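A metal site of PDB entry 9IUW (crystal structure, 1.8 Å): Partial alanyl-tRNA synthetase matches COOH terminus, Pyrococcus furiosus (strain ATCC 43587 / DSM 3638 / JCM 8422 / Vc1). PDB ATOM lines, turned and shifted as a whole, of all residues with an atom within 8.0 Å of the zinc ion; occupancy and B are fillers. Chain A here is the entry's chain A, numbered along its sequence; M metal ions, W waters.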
ATOM      1  N   TYR A  35      -2.261  31.319  12.532  1.00  0.00           N
ATOM      2  CA  TYR A  35      -2.113  30.716  11.208  1.00  0.00           C
ATOM      3  C   TYR A  35      -3.444  30.115  10.756  1.00  0.00           C
ATOM      4  O   TYR A  35      -4.025  29.290  11.484  1.00  0.00           O
ATOM      5  CB  TYR A  35      -1.016  29.658  11.245  1.00  0.00           C
ATOM      6  CG  TYR A  35      -0.798  28.968   9.912  1.00  0.00           C
ATOM      7  CD1 TYR A  35      -0.087  29.601   8.899  1.00  0.00           C
ATOM      8  CD2 TYR A  35      -1.307  27.699   9.684  1.00  0.00           C
ATOM      9  CE1 TYR A  35       0.109  28.980   7.675  1.00  0.00           C
ATOM     10  CE2 TYR A  35      -1.120  27.076   8.470  1.00  0.00           C
ATOM     11  CZ  TYR A  35      -0.412  27.709   7.475  1.00  0.00           C
ATOM     12  OH  TYR A  35      -0.225  27.086   6.261  1.00  0.00           O
ATOM     13  N   GLY A  38      -4.065  25.736   5.961  1.00  0.00           N
ATOM     14  CA  GLY A  38      -3.580  25.715   4.581  1.00  0.00           C
ATOM     15  C   GLY A  38      -2.265  24.983   4.481  1.00  0.00           C
ATOM     16  O   GLY A  38      -1.517  24.852   5.454  1.00  0.00           O
ATOM     17  N   GLY A  39      -1.990  24.486   3.265  1.00  0.00           N
ATOM     18  CA  GLY A  39      -0.711  23.853   3.004  1.00  0.00           C
ATOM     19  C   GLY A  39      -0.484  22.545   3.727  1.00  0.00           C
ATOM     20  O   GLY A  39       0.677  22.129   3.893  1.00  0.00           O
ATOM     21  N   GLY A  40      -1.551  21.887   4.166  1.00  0.00           N
ATOM     22  CA  GLY A  40      -1.471  20.694   4.987  1.00  0.00           C
ATOM     23  C   GLY A  40      -1.277  20.942   6.471  1.00  0.00           C
ATOM     24  O   GLY A  40      -1.302  19.980   7.249  1.00  0.00           O
ATOM     25  N   GLN A  41      -1.070  22.214   6.897  1.00  0.00           N
ATOM     26  CA  GLN A  41      -0.859  22.552   8.298  1.00  0.00           C
ATOM     27  C   GLN A  41      -2.168  23.050   8.912  1.00  0.00           C
ATOM     28  O   GLN A  41      -2.760  23.994   8.388  1.00  0.00           O
ATOM     29  CB  GLN A  41       0.214  23.633   8.447  1.00  0.00           C
ATOM     30  CG  GLN A  41       0.627  23.919   9.897  1.00  0.00           C
ATOM     31  CD  GLN A  41       1.624  25.056  10.026  1.00  0.00           C
ATOM     32  OE1 GLN A  41       2.540  25.191   9.216  1.00  0.00           O
ATOM     33  NE2 GLN A  41       1.464  25.872  11.067  1.00  0.00           N
ATOM     34  N   ILE A  95       7.028  19.621  13.121  1.00  0.00           N
ATOM     35  CA  ILE A  95       6.597  18.568  12.209  1.00  0.00           C
ATOM     36  C   ILE A  95       6.603  19.069  10.777  1.00  0.00           C
ATOM     37  O   ILE A  95       7.008  18.354   9.853  1.00  0.00           O
ATOM     38  CB  ILE A  95       5.215  18.032  12.614  1.00  0.00           C
ATOM     39  CG1 ILE A  95       5.349  17.256  13.931  1.00  0.00           C
ATOM     40  CG2 ILE A  95       4.646  17.123  11.506  1.00  0.00           C
ATOM     41  CD1 ILE A  95       4.015  16.854  14.549  1.00  0.00           C
ATOM     42  N   HIS A  96       6.214  20.316  10.573  1.00  0.00           N
ATOM     43  CA  HIS A  96       6.223  20.854   9.218  1.00  0.00           C
ATOM     44  C   HIS A  96       7.632  20.904   8.671  1.00  0.00           C
ATOM     45  O   HIS A  96       7.902  20.471   7.549  1.00  0.00           O
ATOM     46  CB  HIS A  96       5.582  22.231   9.204  1.00  0.00           C
ATOM     47  CG  HIS A  96       5.076  22.626   7.862  1.00  0.00           C
ATOM     48  ND1 HIS A  96       4.096  23.579   7.681  1.00  0.00           N
ATOM     49  CD2 HIS A  96       5.401  22.183   6.625  1.00  0.00           C
ATOM     50  CE1 HIS A  96       3.841  23.716   6.397  1.00  0.00           C
ATOM     51  NE2 HIS A  96       4.625  22.886   5.732  1.00  0.00           N
ATOM     52  N   SER A  97       8.566  21.418   9.469  1.00  0.00           N
ATOM     53  CA  SER A  97       9.954  21.457   9.007  1.00  0.00           C
ATOM     54  C   SER A  97      10.518  20.049   8.828  1.00  0.00           C
ATOM     55  O   SER A  97      11.315  19.834   7.912  1.00  0.00           O
ATOM     56  CB  SER A  97      10.792  22.305   9.963  1.00  0.00           C
ATOM     57  OG  SER A  97      10.292  23.646   9.986  1.00  0.00           O
ATOM     58  N   LEU A  99       8.841  17.482   7.692  1.00  0.00           N
ATOM     59  CA  LEU A  99       8.366  17.025   6.387  1.00  0.00           C
ATOM     60  C   LEU A  99       9.217  17.578   5.246  1.00  0.00           C
ATOM     61  O   LEU A  99       9.537  16.868   4.293  1.00  0.00           O
ATOM     62  CB  LEU A  99       6.900  17.407   6.167  1.00  0.00           C
ATOM     63  CG  LEU A  99       5.910  16.542   6.938  1.00  0.00           C
ATOM     64  CD1 LEU A  99       4.523  17.223   6.934  1.00  0.00           C
ATOM     65  CD2 LEU A  99       5.811  15.126   6.342  1.00  0.00           C
ATOM     66  N   HIS A 100       9.625  18.854   5.344  1.00  0.00           N
ATOM     67  CA  HIS A 100      10.536  19.421   4.357  1.00  0.00           C
ATOM     68  C   HIS A 100      11.889  18.718   4.385  1.00  0.00           C
ATOM     69  O   HIS A 100      12.440  18.365   3.332  1.00  0.00           O
ATOM     70  CB  HIS A 100      10.727  20.912   4.605  1.00  0.00           C
ATOM     71  CG  HIS A 100       9.555  21.737   4.185  1.00  0.00           C
ATOM     72  ND1 HIS A 100       9.696  22.992   3.617  1.00  0.00           N
ATOM     73  CD2 HIS A 100       8.226  21.492   4.237  1.00  0.00           C
ATOM     74  CE1 HIS A 100       8.498  23.487   3.355  1.00  0.00           C
ATOM     75  NE2 HIS A 100       7.589  22.593   3.710  1.00  0.00           N
ATOM     76  N   GLU A 103      11.686  15.406   2.750  1.00  0.00           N
ATOM     77  CA  GLU A 103      11.681  15.493   1.259  1.00  0.00           C
ATOM     78  C   GLU A 103      13.119  15.657   0.731  1.00  0.00           C
ATOM     79  O   GLU A 103      13.491  14.958  -0.191  1.00  0.00           O
ATOM     80  CB  GLU A 103      10.813  16.647   0.743  1.00  0.00           C
ATOM     81  CG  GLU A 103       9.336  16.452   1.026  1.00  0.00           C
ATOM     82  CD  GLU A 103       8.509  17.644   0.575  1.00  0.00           C
ATOM     83  OE1 GLU A 103       7.710  18.133   1.405  1.00  0.00           O
ATOM     84  OE2 GLU A 103       8.697  18.075  -0.578  1.00  0.00           O
ATOM     85  N   SER A 120       0.622  15.572   1.163  1.00  0.00           N
ATOM     86  CA  SER A 120       1.363  16.033   2.336  1.00  0.00           C
ATOM     87  C   SER A 120       0.360  16.588   3.349  1.00  0.00           C
ATOM     88  O   SER A 120      -0.564  17.291   2.960  1.00  0.00           O
ATOM     89  CB  SER A 120       2.384  17.116   1.953  1.00  0.00           C
ATOM     90  OG  SER A 120       3.284  17.378   3.003  1.00  0.00           O
ATOM     91  N   MET A 122      -0.325  17.130   8.054  1.00  0.00           N
ATOM     92  CA  MET A 122       0.201  16.905   9.396  1.00  0.00           C
ATOM     93  C   MET A 122      -0.872  17.172  10.428  1.00  0.00           C
ATOM     94  O   MET A 122      -1.840  17.888  10.185  1.00  0.00           O
ATOM     95  CB  MET A 122       1.421  17.800   9.666  1.00  0.00           C
ATOM     96  CG  MET A 122       1.042  19.274   9.562  1.00  0.00           C
ATOM     97  SD  MET A 122       2.457  20.359   9.339  1.00  0.00           S
ATOM     98  CE  MET A 122       2.399  20.448   7.567  1.00  0.00           C
ATOM     99  N   ARG A 167       5.279  31.273  -1.251  1.00  0.00           N
ATOM    100  CA  ARG A 167       6.332  31.379  -0.225  1.00  0.00           C
ATOM    101  C   ARG A 167       7.269  30.186  -0.400  1.00  0.00           C
ATOM    102  O   ARG A 167       6.774  29.086  -0.651  1.00  0.00           O
ATOM    103  CB  ARG A 167       5.705  31.364   1.164  1.00  0.00           C
ATOM    104  CG  ARG A 167       6.627  31.905   2.247  1.00  0.00           C
ATOM    105  CD  ARG A 167       5.981  31.756   3.613  1.00  0.00           C
ATOM    106  NE  ARG A 167       6.609  32.568   4.650  1.00  0.00           N
ATOM    107  CZ  ARG A 167       6.994  32.133   5.835  1.00  0.00           C
ATOM    108  NH1 ARG A 167       6.938  30.851   6.146  1.00  0.00           N
ATOM    109  NH2 ARG A 167       7.459  33.005   6.724  1.00  0.00           N
ATOM    110  N   THR A 169      10.752  28.015   1.148  1.00  0.00           N
ATOM    111  CA  THR A 169      11.598  27.703   2.294  1.00  0.00           C
ATOM    112  C   THR A 169      12.761  26.880   1.786  1.00  0.00           C
ATOM    113  O   THR A 169      12.631  26.106   0.834  1.00  0.00           O
ATOM    114  CB  THR A 169      10.861  26.906   3.369  1.00  0.00           C
ATOM    115  OG1 THR A 169      10.411  25.684   2.806  1.00  0.00           O
ATOM    116  CG2 THR A 169       9.642  27.660   3.891  1.00  0.00           C
ATOM    117  N   ILE A 177      11.604  24.441  -1.252  1.00  0.00           N
ATOM    118  CA  ILE A 177      10.289  23.816  -1.248  1.00  0.00           C
ATOM    119  C   ILE A 177       9.221  24.889  -1.071  1.00  0.00           C
ATOM    120  O   ILE A 177       9.192  25.573  -0.050  1.00  0.00           O
ATOM    121  CB  ILE A 177      10.146  22.759  -0.151  1.00  0.00           C
ATOM    122  CG1 ILE A 177      11.130  21.611  -0.400  1.00  0.00           C
ATOM    123  CG2 ILE A 177       8.729  22.236  -0.077  1.00  0.00           C
ATOM    124  CD1 ILE A 177      11.334  20.712   0.813  1.00  0.00           C
ATOM    125  N   PRO A 178       8.369  25.178  -2.101  1.00  0.00           N
ATOM    126  CA  PRO A 178       7.383  26.246  -1.994  1.00  0.00           C
ATOM    127  C   PRO A 178       6.159  25.780  -1.228  1.00  0.00           C
ATOM    128  O   PRO A 178       5.606  24.712  -1.586  1.00  0.00           O
ATOM    129  CB  PRO A 178       7.010  26.596  -3.436  1.00  0.00           C
ATOM    130  CG  PRO A 178       7.227  25.317  -4.200  1.00  0.00           C
ATOM    131  CD  PRO A 178       8.281  24.541  -3.434  1.00  0.00           C
ATOM    132  N   CYS A 179       5.724  26.582  -0.248  1.00  0.00           N
ATOM    133  CA  CYS A 179       4.507  26.226   0.515  1.00  0.00           C
ATOM    134  C   CYS A 179       4.217  27.239   1.619  1.00  0.00           C
ATOM    135  O   CYS A 179       5.166  27.928   2.057  1.00  0.00           O
ATOM    136  CB  CYS A 179       4.680  24.871   1.188  1.00  0.00           C
ATOM    137  SG  CYS A 179       5.383  24.958   2.848  1.00  0.00           S
ATOM    138  N   GLY A 180       2.956  27.320   2.055  1.00  0.00           N
ATOM    139  CA  GLY A 180       2.610  28.199   3.189  1.00  0.00           C
ATOM    140  C   GLY A 180       2.715  27.418   4.479  1.00  0.00           C
ATOM    141  O   GLY A 180       2.637  26.174   4.409  1.00  0.00           O
ATOM    142  N   GLY A 181       2.864  28.096   5.623  1.00  0.00           N
ATOM    143  CA  GLY A 181       3.053  27.389   6.867  1.00  0.00           C
ATOM    144  C   GLY A 181       4.248  27.906   7.626  1.00  0.00           C
ATOM    145  O   GLY A 181       5.067  28.672   7.115  1.00  0.00           O
ATOM    146  N   THR A 182       4.322  27.485   8.885  1.00  0.00           N
ATOM    147  CA  THR A 182       5.244  28.055   9.858  1.00  0.00           C
ATOM    148  C   THR A 182       6.338  27.033  10.140  1.00  0.00           C
ATOM    149  O   THR A 182       6.032  25.866  10.408  1.00  0.00           O
ATOM    150  CB  THR A 182       4.516  28.437  11.149  1.00  0.00           C
ATOM    151  OG1 THR A 182       3.871  27.274  11.668  1.00  0.00           O
ATOM    152  CG2 THR A 182       3.476  29.536  10.882  1.00  0.00           C
ATOM    153  N   HIS A 183       7.583  27.477  10.087  1.00  0.00           N
ATOM    154  CA  HIS A 183       8.738  26.597  10.200  1.00  0.00           C
ATOM    155  C   HIS A 183       9.614  27.028  11.356  1.00  0.00           C
ATOM    156  O   HIS A 183       9.596  28.188  11.778  1.00  0.00           O
ATOM    157  CB  HIS A 183       9.537  26.598   8.899  1.00  0.00           C
ATOM    158  CG  HIS A 183       8.854  25.860   7.785  1.00  0.00           C
ATOM    159  ND1 HIS A 183       9.018  24.507   7.589  1.00  0.00           N
ATOM    160  CD2 HIS A 183       7.980  26.275   6.837  1.00  0.00           C
ATOM    161  CE1 HIS A 183       8.270  24.110   6.585  1.00  0.00           C
ATOM    162  NE2 HIS A 183       7.637  25.169   6.093  1.00  0.00           N
HETATM  163 ZN    ZN M   1       5.360  22.747   3.620  1.00  0.00          ZN
HETATM  164  O   HOH W   1       5.000  20.600   3.502  1.00  0.00           O
HETATM  165  O   HOH W   2       3.152  23.228   3.056  1.00  0.00           O
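A ring nitrogen (ND1) of His 100 is in hydrogen-bond range of the side-chain hydroxyl (OG1) of Thr 169, 2.9 Å away. The side-chain amide oxygen of Gln 41 lies within hydrogen-bond range of a ring nitrogen (ND1) of His 96, 2.7 Å away. The backbone NH (N) of Cys 179 lies within hydrogen-bond range of the backbone carbonyl oxygen (O) of Arg 167 (2.7 Å).
Of the 22 residues printed, 3 come within 4 Å of the zinc ion. The nearest printed residue that does not touch the zinc ion is His 183 (4.1 Å).
The zinc ion is bound by water W1 (2.2 Å), NE2 of His 100 (2.2 Å), NE2 of His 96 (2.2 Å), water W2 (2.3 Å) and SG of Cys 179 (2.3 Å).
Water W2 lies within hydrogen-bond range of O of Gly 39 (2.8 Å) and O of Gly 180 (3.3 Å).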
